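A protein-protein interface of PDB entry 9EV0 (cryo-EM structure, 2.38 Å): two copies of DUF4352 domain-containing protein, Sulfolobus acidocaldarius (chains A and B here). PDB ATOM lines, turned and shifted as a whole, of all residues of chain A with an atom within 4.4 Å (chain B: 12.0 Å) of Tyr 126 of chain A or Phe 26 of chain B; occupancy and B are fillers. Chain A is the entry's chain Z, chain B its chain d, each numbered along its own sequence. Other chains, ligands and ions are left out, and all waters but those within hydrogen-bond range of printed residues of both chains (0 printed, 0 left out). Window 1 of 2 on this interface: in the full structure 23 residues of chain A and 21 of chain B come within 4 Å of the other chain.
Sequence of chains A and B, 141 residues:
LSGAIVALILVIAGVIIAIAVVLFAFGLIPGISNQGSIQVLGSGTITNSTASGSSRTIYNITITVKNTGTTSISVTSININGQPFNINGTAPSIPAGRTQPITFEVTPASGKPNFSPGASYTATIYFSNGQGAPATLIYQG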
ATOM      1  N   GLN A  35     -24.985 -24.019  32.017  1.00  0.00           N
ATOM      2  CA  GLN A  35     -24.147 -22.912  31.556  1.00  0.00           C
ATOM      3  C   GLN A  35     -24.660 -21.545  32.032  1.00  0.00           C
ATOM      4  O   GLN A  35     -23.900 -20.582  32.048  1.00  0.00           O
ATOM      5  CB  GLN A  35     -24.073 -22.972  30.023  1.00  0.00           C
ATOM      6  CG  GLN A  35     -23.074 -22.027  29.362  1.00  0.00           C
ATOM      7  CD  GLN A  35     -21.660 -22.315  29.795  1.00  0.00           C
ATOM      8  OE1 GLN A  35     -20.965 -23.166  29.244  1.00  0.00           O
ATOM      9  NE2 GLN A  35     -21.215 -21.614  30.820  1.00  0.00           N
ATOM     10  N   SER A  74     -18.880 -22.064  42.444  1.00  0.00           N
ATOM     11  CA  SER A  74     -17.931 -21.166  43.093  1.00  0.00           C
ATOM     12  C   SER A  74     -17.428 -20.068  42.147  1.00  0.00           C
ATOM     13  O   SER A  74     -17.396 -20.236  40.931  1.00  0.00           O
ATOM     14  CB  SER A  74     -16.786 -21.944  43.709  1.00  0.00           C
ATOM     15  OG  SER A  74     -16.072 -22.660  42.708  1.00  0.00           O
ATOM     16  N   VAL A  75     -17.032 -18.931  42.729  1.00  0.00           N
ATOM     17  CA  VAL A  75     -16.347 -17.874  41.997  1.00  0.00           C
ATOM     18  C   VAL A  75     -14.925 -18.336  41.675  1.00  0.00           C
ATOM     19  O   VAL A  75     -14.146 -18.630  42.572  1.00  0.00           O
ATOM     20  CB  VAL A  75     -16.332 -16.565  42.808  1.00  0.00           C
ATOM     21  CG1 VAL A  75     -15.484 -15.494  42.135  1.00  0.00           C
ATOM     22  CG2 VAL A  75     -17.738 -16.054  43.051  1.00  0.00           C
ATOM     23  N   THR A  76     -14.568 -18.374  40.387  1.00  0.00           N
ATOM     24  CA  THR A  76     -13.241 -18.790  39.941  1.00  0.00           C
ATOM     25  C   THR A  76     -12.299 -17.601  39.750  1.00  0.00           C
ATOM     26  O   THR A  76     -11.120 -17.689  40.101  1.00  0.00           O
ATOM     27  CB  THR A  76     -13.296 -19.615  38.653  1.00  0.00           C
ATOM     28  OG1 THR A  76     -13.833 -18.848  37.578  1.00  0.00           O
ATOM     29  CG2 THR A  76     -14.114 -20.873  38.806  1.00  0.00           C
ATOM     30  N   SER A  77     -12.823 -16.494  39.210  1.00  0.00           N
ATOM     31  CA  SER A  77     -12.060 -15.281  38.963  1.00  0.00           C
ATOM     32  C   SER A  77     -12.991 -14.076  38.863  1.00  0.00           C
ATOM     33  O   SER A  77     -14.201 -14.207  38.711  1.00  0.00           O
ATOM     34  CB  SER A  77     -11.184 -15.411  37.734  1.00  0.00           C
ATOM     35  OG  SER A  77     -11.956 -15.461  36.541  1.00  0.00           O
ATOM     36  N   THR A 124     -17.078  -8.263  36.319  1.00  0.00           N
ATOM     37  CA  THR A 124     -17.591  -9.519  35.803  1.00  0.00           C
ATOM     38  C   THR A 124     -17.050 -10.614  36.700  1.00  0.00           C
ATOM     39  O   THR A 124     -15.839 -10.755  36.864  1.00  0.00           O
ATOM     40  CB  THR A 124     -17.194  -9.785  34.348  1.00  0.00           C
ATOM     41  OG1 THR A 124     -15.780  -9.941  34.288  1.00  0.00           O
ATOM     42  CG2 THR A 124     -17.581  -8.654  33.425  1.00  0.00           C
ATOM     43  N   ILE A 125     -17.961 -11.373  37.294  1.00  0.00           N
ATOM     44  CA  ILE A 125     -17.587 -12.474  38.155  1.00  0.00           C
ATOM     45  C   ILE A 125     -17.725 -13.736  37.310  1.00  0.00           C
ATOM     46  O   ILE A 125     -18.753 -13.926  36.664  1.00  0.00           O
ATOM     47  CB  ILE A 125     -18.445 -12.484  39.437  1.00  0.00           C
ATOM     48  CG1 ILE A 125     -18.399 -11.136  40.168  1.00  0.00           C
ATOM     49  CG2 ILE A 125     -17.968 -13.580  40.365  1.00  0.00           C
ATOM     50  CD1 ILE A 125     -19.557 -10.207  39.884  1.00  0.00           C
ATOM     51  N   TYR A 126     -16.674 -14.559  37.273  1.00  0.00           N
ATOM     52  CA  TYR A 126     -16.676 -15.794  36.509  1.00  0.00           C
ATOM     53  C   TYR A 126     -16.803 -16.981  37.450  1.00  0.00           C
ATOM     54  O   TYR A 126     -15.994 -17.179  38.350  1.00  0.00           O
ATOM     55  CB  TYR A 126     -15.417 -15.895  35.650  1.00  0.00           C
ATOM     56  CG  TYR A 126     -15.429 -14.963  34.470  1.00  0.00           C
ATOM     57  CD1 TYR A 126     -16.172 -15.268  33.337  1.00  0.00           C
ATOM     58  CD2 TYR A 126     -14.716 -13.771  34.494  1.00  0.00           C
ATOM     59  CE1 TYR A 126     -16.198 -14.415  32.243  1.00  0.00           C
ATOM     60  CE2 TYR A 126     -14.742 -12.899  33.410  1.00  0.00           C
ATOM     61  CZ  TYR A 126     -15.477 -13.227  32.280  1.00  0.00           C
ATOM     62  OH  TYR A 126     -15.503 -12.399  31.193  1.00  0.00           O
ATOM     63  N   PHE A 127     -17.826 -17.793  37.203  1.00  0.00           N
ATOM     64  CA  PHE A 127     -18.187 -18.919  38.054  1.00  0.00           C
ATOM     65  C   PHE A 127     -17.670 -20.237  37.472  1.00  0.00           C
ATOM     66  O   PHE A 127     -17.288 -20.296  36.309  1.00  0.00           O
ATOM     67  CB  PHE A 127     -19.702 -18.886  38.244  1.00  0.00           C
ATOM     68  CG  PHE A 127     -20.172 -17.634  38.949  1.00  0.00           C
ATOM     69  CD1 PHE A 127     -20.251 -17.586  40.337  1.00  0.00           C
ATOM     70  CD2 PHE A 127     -20.490 -16.484  38.230  1.00  0.00           C
ATOM     71  CE1 PHE A 127     -20.659 -16.425  40.984  1.00  0.00           C
ATOM     72  CE2 PHE A 127     -20.879 -15.316  38.878  1.00  0.00           C
ATOM     73  CZ  PHE A 127     -20.968 -15.292  40.255  1.00  0.00           C
ATOM     74  N   GLY A 130     -17.818 -21.681  33.910  1.00  0.00           N
ATOM     75  CA  GLY A 130     -17.281 -20.827  32.857  1.00  0.00           C
ATOM     76  C   GLY A 130     -18.157 -19.609  32.535  1.00  0.00           C
ATOM     77  O   GLY A 130     -17.746 -18.737  31.766  1.00  0.00           O
ATOM     78  N   GLN A 131     -19.349 -19.528  33.150  1.00  0.00           N
ATOM     79  CA  GLN A 131     -20.292 -18.421  33.002  1.00  0.00           C
ATOM     80  C   GLN A 131     -19.728 -17.138  33.617  1.00  0.00           C
ATOM     81  O   GLN A 131     -19.262 -17.153  34.754  1.00  0.00           O
ATOM     82  CB  GLN A 131     -21.593 -18.801  33.715  1.00  0.00           C
ATOM     83  CG  GLN A 131     -22.717 -17.796  33.515  1.00  0.00           C
ATOM     84  CD  GLN A 131     -23.953 -18.082  34.335  1.00  0.00           C
ATOM     85  OE1 GLN A 131     -24.043 -19.044  35.091  1.00  0.00           O
ATOM     86  NE2 GLN A 131     -24.949 -17.224  34.209  1.00  0.00           N
ATOM     87  N   GLY A 132     -19.826 -16.023  32.882  1.00  0.00           N
ATOM     88  CA  GLY A 132     -19.514 -14.708  33.419  1.00  0.00           C
ATOM     89  C   GLY A 132     -20.768 -13.854  33.577  1.00  0.00           C
ATOM     90  O   GLY A 132     -21.552 -13.731  32.640  1.00  0.00           O
ATOM     91  N   VAL B  15     -22.003 -29.029  19.811  1.00  0.00           N
ATOM     92  CA  VAL B  15     -22.029 -28.657  21.225  1.00  0.00           C
ATOM     93  C   VAL B  15     -20.726 -27.960  21.618  1.00  0.00           C
ATOM     94  O   VAL B  15     -20.762 -26.887  22.206  1.00  0.00           O
ATOM     95  CB  VAL B  15     -22.306 -29.881  22.121  1.00  0.00           C
ATOM     96  CG1 VAL B  15     -22.142 -29.589  23.610  1.00  0.00           C
ATOM     97  CG2 VAL B  15     -23.693 -30.441  21.865  1.00  0.00           C
ATOM     98  N   ILE B  16     -19.586 -28.543  21.246  1.00  0.00           N
ATOM     99  CA  ILE B  16     -18.258 -28.043  21.573  1.00  0.00           C
ATOM    100  C   ILE B  16     -18.038 -26.635  21.011  1.00  0.00           C
ATOM    101  O   ILE B  16     -17.666 -25.731  21.750  1.00  0.00           O
ATOM    102  CB  ILE B  16     -17.194 -29.046  21.086  1.00  0.00           C
ATOM    103  CG1 ILE B  16     -17.290 -30.360  21.859  1.00  0.00           C
ATOM    104  CG2 ILE B  16     -15.781 -28.463  21.158  1.00  0.00           C
ATOM    105  CD1 ILE B  16     -16.651 -31.543  21.151  1.00  0.00           C
ATOM    106  N   ILE B  17     -18.292 -26.433  19.715  1.00  0.00           N
ATOM    107  CA  ILE B  17     -18.064 -25.151  19.058  1.00  0.00           C
ATOM    108  C   ILE B  17     -19.094 -24.104  19.501  1.00  0.00           C
ATOM    109  O   ILE B  17     -18.743 -22.946  19.688  1.00  0.00           O
ATOM    110  CB  ILE B  17     -17.955 -25.337  17.527  1.00  0.00           C
ATOM    111  CG1 ILE B  17     -16.698 -26.142  17.187  1.00  0.00           C
ATOM    112  CG2 ILE B  17     -17.951 -24.004  16.780  1.00  0.00           C
ATOM    113  CD1 ILE B  17     -16.716 -26.812  15.822  1.00  0.00           C
ATOM    114  N   ALA B  18     -20.350 -24.494  19.748  1.00  0.00           N
ATOM    115  CA  ALA B  18     -21.351 -23.579  20.282  1.00  0.00           C
ATOM    116  C   ALA B  18     -20.977 -23.101  21.691  1.00  0.00           C
ATOM    117  O   ALA B  18     -20.961 -21.898  21.942  1.00  0.00           O
ATOM    118  CB  ALA B  18     -22.720 -24.213  20.228  1.00  0.00           C
ATOM    119  N   ILE B  19     -20.597 -24.013  22.589  1.00  0.00           N
ATOM    120  CA  ILE B  19     -20.154 -23.647  23.931  1.00  0.00           C
ATOM    121  C   ILE B  19     -18.893 -22.783  23.879  1.00  0.00           C
ATOM    122  O   ILE B  19     -18.820 -21.794  24.597  1.00  0.00           O
ATOM    123  CB  ILE B  19     -20.015 -24.888  24.834  1.00  0.00           C
ATOM    124  CG1 ILE B  19     -21.403 -25.458  25.128  1.00  0.00           C
ATOM    125  CG2 ILE B  19     -19.261 -24.572  26.126  1.00  0.00           C
ATOM    126  CD1 ILE B  19     -21.399 -26.790  25.852  1.00  0.00           C
ATOM    127  N   ALA B  20     -17.939 -23.078  22.990  1.00  0.00           N
ATOM    128  CA  ALA B  20     -16.755 -22.242  22.801  1.00  0.00           C
ATOM    129  C   ALA B  20     -17.121 -20.797  22.426  1.00  0.00           C
ATOM    130  O   ALA B  20     -16.562 -19.855  22.986  1.00  0.00           O
ATOM    131  CB  ALA B  20     -15.843 -22.887  21.785  1.00  0.00           C
ATOM    132  N   VAL B  21     -18.092 -20.602  21.528  1.00  0.00           N
ATOM    133  CA  VAL B  21     -18.575 -19.279  21.139  1.00  0.00           C
ATOM    134  C   VAL B  21     -19.373 -18.600  22.261  1.00  0.00           C
ATOM    135  O   VAL B  21     -19.277 -17.387  22.428  1.00  0.00           O
ATOM    136  CB  VAL B  21     -19.350 -19.354  19.808  1.00  0.00           C
ATOM    137  CG1 VAL B  21     -20.105 -18.073  19.470  1.00  0.00           C
ATOM    138  CG2 VAL B  21     -18.401 -19.697  18.678  1.00  0.00           C
ATOM    139  N   VAL B  22     -20.112 -19.355  23.079  1.00  0.00           N
ATOM    140  CA  VAL B  22     -20.807 -18.822  24.248  1.00  0.00           C
ATOM    141  C   VAL B  22     -19.822 -18.356  25.327  1.00  0.00           C
ATOM    142  O   VAL B  22     -19.966 -17.261  25.863  1.00  0.00           O
ATOM    143  CB  VAL B  22     -21.812 -19.858  24.778  1.00  0.00           C
ATOM    144  CG1 VAL B  22     -22.369 -19.508  26.154  1.00  0.00           C
ATOM    145  CG2 VAL B  22     -22.949 -20.028  23.789  1.00  0.00           C
ATOM    146  N   LEU B  23     -18.781 -19.147  25.611  1.00  0.00           N
ATOM    147  CA  LEU B  23     -17.708 -18.764  26.523  1.00  0.00           C
ATOM    148  C   LEU B  23     -16.942 -17.545  26.009  1.00  0.00           C
ATOM    149  O   LEU B  23     -16.617 -16.659  26.791  1.00  0.00           O
ATOM    150  CB  LEU B  23     -16.757 -19.944  26.726  1.00  0.00           C
ATOM    151  CG  LEU B  23     -17.324 -21.122  27.509  1.00  0.00           C
ATOM    152  CD1 LEU B  23     -16.379 -22.302  27.405  1.00  0.00           C
ATOM    153  CD2 LEU B  23     -17.554 -20.756  28.971  1.00  0.00           C
ATOM    154  N   PHE B  24     -16.698 -17.452  24.699  1.00  0.00           N
ATOM    155  CA  PHE B  24     -16.120 -16.262  24.096  1.00  0.00           C
ATOM    156  C   PHE B  24     -17.002 -15.027  24.312  1.00  0.00           C
ATOM    157  O   PHE B  24     -16.489 -13.985  24.716  1.00  0.00           O
ATOM    158  CB  PHE B  24     -15.835 -16.509  22.617  1.00  0.00           C
ATOM    159  CG  PHE B  24     -15.334 -15.291  21.876  1.00  0.00           C
ATOM    160  CD1 PHE B  24     -13.989 -14.938  21.908  1.00  0.00           C
ATOM    161  CD2 PHE B  24     -16.207 -14.477  21.160  1.00  0.00           C
ATOM    162  CE1 PHE B  24     -13.525 -13.818  21.228  1.00  0.00           C
ATOM    163  CE2 PHE B  24     -15.745 -13.354  20.487  1.00  0.00           C
ATOM    164  CZ  PHE B  24     -14.407 -13.021  20.528  1.00  0.00           C
ATOM    165  N   ALA B  25     -18.321 -15.137  24.105  1.00  0.00           N
ATOM    166  CA  ALA B  25     -19.240 -14.036  24.366  1.00  0.00           C
ATOM    167  C   ALA B  25     -19.190 -13.579  25.832  1.00  0.00           C
ATOM    168  O   ALA B  25     -19.114 -12.381  26.084  1.00  0.00           O
ATOM    169  CB  ALA B  25     -20.628 -14.402  23.903  1.00  0.00           C
ATOM    170  N   PHE B  26     -19.143 -14.497  26.809  1.00  0.00           N
ATOM    171  CA  PHE B  26     -18.909 -14.115  28.202  1.00  0.00           C
ATOM    172  C   PHE B  26     -17.535 -13.472  28.429  1.00  0.00           C
ATOM    173  O   PHE B  26     -17.400 -12.612  29.296  1.00  0.00           O
ATOM    174  CB  PHE B  26     -19.036 -15.323  29.132  1.00  0.00           C
ATOM    175  CG  PHE B  26     -20.420 -15.904  29.304  1.00  0.00           C
ATOM    176  CD1 PHE B  26     -21.469 -15.115  29.767  1.00  0.00           C
ATOM    177  CD2 PHE B  26     -20.669 -17.252  29.051  1.00  0.00           C
ATOM    178  CE1 PHE B  26     -22.736 -15.649  29.957  1.00  0.00           C
ATOM    179  CE2 PHE B  26     -21.934 -17.791  29.273  1.00  0.00           C
ATOM    180  CZ  PHE B  26     -22.967 -16.985  29.705  1.00  0.00           C
ATOM    181  N   GLY B  27     -16.511 -13.885  27.673  1.00  0.00           N
ATOM    182  CA  GLY B  27     -15.158 -13.349  27.757  1.00  0.00           C
ATOM    183  C   GLY B  27     -15.004 -11.936  27.190  1.00  0.00           C
ATOM    184  O   GLY B  27     -14.080 -11.230  27.580  1.00  0.00           O
ATOM    185  N   LEU B  28     -15.917 -11.489  26.313  1.00  0.00           N
ATOM    186  CA  LEU B  28     -15.934 -10.123  25.798  1.00  0.00           C
ATOM    187  C   LEU B  28     -16.384  -9.110  26.845  1.00  0.00           C
ATOM    188  O   LEU B  28     -15.952  -7.963  26.803  1.00  0.00           O
ATOM    189  CB  LEU B  28     -16.890 -10.022  24.612  1.00  0.00           C
ATOM    190  CG  LEU B  28     -16.379 -10.587  23.298  1.00  0.00           C
ATOM    191  CD1 LEU B  28     -17.540 -10.672  22.328  1.00  0.00           C
ATOM    192  CD2 LEU B  28     -15.276  -9.708  22.720  1.00  0.00           C
ATOM    193  N   ILE B  29     -17.263  -9.518  27.764  1.00  0.00           N
ATOM    194  CA  ILE B  29     -17.976  -8.617  28.661  1.00  0.00           C
ATOM    195  C   ILE B  29     -17.048  -7.648  29.405  1.00  0.00           C
ATOM    196  O   ILE B  29     -17.350  -6.466  29.422  1.00  0.00           O
ATOM    197  CB  ILE B  29     -18.942  -9.400  29.578  1.00  0.00           C
ATOM    198  CG1 ILE B  29     -19.973 -10.163  28.739  1.00  0.00           C
ATOM    199  CG2 ILE B  29     -19.623  -8.490  30.597  1.00  0.00           C
ATOM    200  CD1 ILE B  29     -20.968 -10.998  29.537  1.00  0.00           C
ATOM    201  N   PRO B  30     -15.896  -8.040  29.999  1.00  0.00           N
ATOM    202  CA  PRO B  30     -15.055  -7.113  30.753  1.00  0.00           C
ATOM    203  C   PRO B  30     -14.457  -5.998  29.903  1.00  0.00           C
ATOM    204  O   PRO B  30     -14.404  -4.855  30.352  1.00  0.00           O
ATOM    205  CB  PRO B  30     -13.930  -7.990  31.325  1.00  0.00           C
ATOM    206  CG  PRO B  30     -14.456  -9.401  31.246  1.00  0.00           C
ATOM    207  CD  PRO B  30     -15.335  -9.384  30.020  1.00  0.00           C
ATOM    208  N   GLY B  31     -14.048  -6.313  28.669  1.00  0.00           N
ATOM    209  CA  GLY B  31     -13.423  -5.353  27.767  1.00  0.00           C
ATOM    210  C   GLY B  31     -14.400  -4.303  27.231  1.00  0.00           C
ATOM    211  O   GLY B  31     -14.036  -3.144  27.078  1.00  0.00           O
ATOM    212  N   ILE B  32     -15.652  -4.695  26.969  1.00  0.00           N
ATOM    213  CA  ILE B  32     -16.662  -3.814  26.387  1.00  0.00           C
ATOM    214  C   ILE B  32     -17.405  -2.975  27.435  1.00  0.00           C
ATOM    215  O   ILE B  32     -18.100  -2.025  27.063  1.00  0.00           O
ATOM    216  CB  ILE B  32     -17.665  -4.615  25.531  1.00  0.00           C
ATOM    217  CG1 ILE B  32     -18.578  -5.494  26.399  1.00  0.00           C
ATOM    218  CG2 ILE B  32     -16.936  -5.396  24.446  1.00  0.00           C
ATOM    219  CD1 ILE B  32     -19.607  -6.303  25.641  1.00  0.00           C
ATOM    220  N   SER B  33     -17.302  -3.312  28.736  1.00  0.00           N
ATOM    221  CA  SER B  33     -18.230  -2.812  29.755  1.00  0.00           C
ATOM    222  C   SER B  33     -17.583  -2.082  30.942  1.00  0.00           C
ATOM    223  O   SER B  33     -18.222  -1.959  31.993  1.00  0.00           O
ATOM    224  CB  SER B  33     -19.150  -3.918  30.236  1.00  0.00           C
ATOM    225  OG  SER B  33     -18.450  -4.839  31.058  1.00  0.00           O
ATOM    226  N   ASN B  34     -16.355  -1.569  30.792  1.00  0.00           N
ATOM    227  CA  ASN B  34     -15.755  -0.749  31.834  1.00  0.00           C
ATOM    228  C   ASN B  34     -16.589   0.518  32.048  1.00  0.00           C
ATOM    229  O   ASN B  34     -16.757   1.332  31.141  1.00  0.00           O
ATOM    230  CB  ASN B  34     -14.267  -0.488  31.569  1.00  0.00           C
ATOM    231  CG  ASN B  34     -13.998   0.322  30.319  1.00  0.00           C
ATOM    232  OD1 ASN B  34     -14.406  -0.066  29.224  1.00  0.00           O
ATOM    233  ND2 ASN B  34     -13.303   1.441  30.466  1.00  0.00           N
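Of chain A, only Tyr 126, Gln 131 and Gly 132 come within 4 Å of Phe 26 of chain B.
Gln 35 of chain A touches one residue of chain B.
No residue of chain B comes within 4 Å of Val 75 of chain A.
No residue of chain B comes within 4 Å of Thr 76 of chain A.
Thr 124 of chain A touches just these residues of chain B: Ile 29 (3.5 Å) and Pro 30 (3.4 Å).
No residue of chain B comes within 4 Å of Ile 125 of chain A.
Of chain B, only Phe 26 comes within 4 Å of Gln 131 of chain A.
Of chain B, only Phe 26 comes within 4 Å of Gly 132 of chain A.
Of the printed residues of chain A, Pro 30 of chain B touches Thr 124 and Tyr 126.
Printed residues of chain A within 4 Å of Ile 29 of chain B: Thr 124.
Leu 28 of chain B touches none of the printed residues of chain A.
The nearest residue of chain B that does not touch Tyr 126 of chain A is Ile 29 of chain B (4.8 Å).
O of Gln 35 of chain A sits close to OE1 of Gln 131 of chain A (3.4 Å).
N of Thr 76 of chain A sits at hydrogen-bond distance from O of Tyr 126 of chain A, 2.8 Å away.
The backbone carbonyl oxygen (O) of Ser 77 of chain A sits at hydrogen-bond distance from the backbone NH (N) of Tyr 126 of chain A, at 2.9 Å.
The backbone carbonyl oxygen (O) of Ile 29 of chain B is in hydrogen-bond range of the side-chain hydroxyl (OG) of Ser 33 of chain B (2.6 Å).
OE1 of Gln 35 of chain A touches CG2 of Ile 19 of chain B (3.8 Å).
Ile 29 of chain B touches Thr 124 of chain A (CG2 to CG2, 3.5 Å).
Pro 30 of chain B touches Thr 124 of chain A.
CA of Gly 27 of chain B touches OH of Tyr 126 of chain A, 3.6 Å away.
Tyr 126 of chain A touches Pro 30 of chain B (OH to CG, 3.2 Å).
Leu 23 of chain B touches Gly 130 of chain A (CD2 to O, 3.5 Å).
Phe 26 of chain B touches Gln 131 of chain A (CZ to CG, 3.9 Å).
Phe 26 of chain B touches Gly 132 of chain A (CD1 to O, 3.2 Å).
No position is printed for both chains.
The side-chain hydroxyl of Tyr 126 of chain A sits at hydrogen-bond distance from the backbone carbonyl oxygen of Phe 26 of chain B, 2.7 Å away.
Printed residues of chain A that touch a printed residue of chain B: Gln 35, Thr 124, Tyr 126, Gly 130, Gln 131 and Gly 132.
Hydrophobic or aromatic side chains of chain A that line the printed part of chain B: Tyr 126.
Of the 20 printed residues of chain B, 6 touch a printed residue of chain A.
Printed residues of chain B that touch a printed residue of chain A: Ile 19, Leu 23, Phe 26, Gly 27, Ile 29 and Pro 30.
Hydrophobic or aromatic side chains of chain B within 4 Å of the printed part of chain A: Ile 19, Leu 23, Phe 26, Ile 29 and Pro 30.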
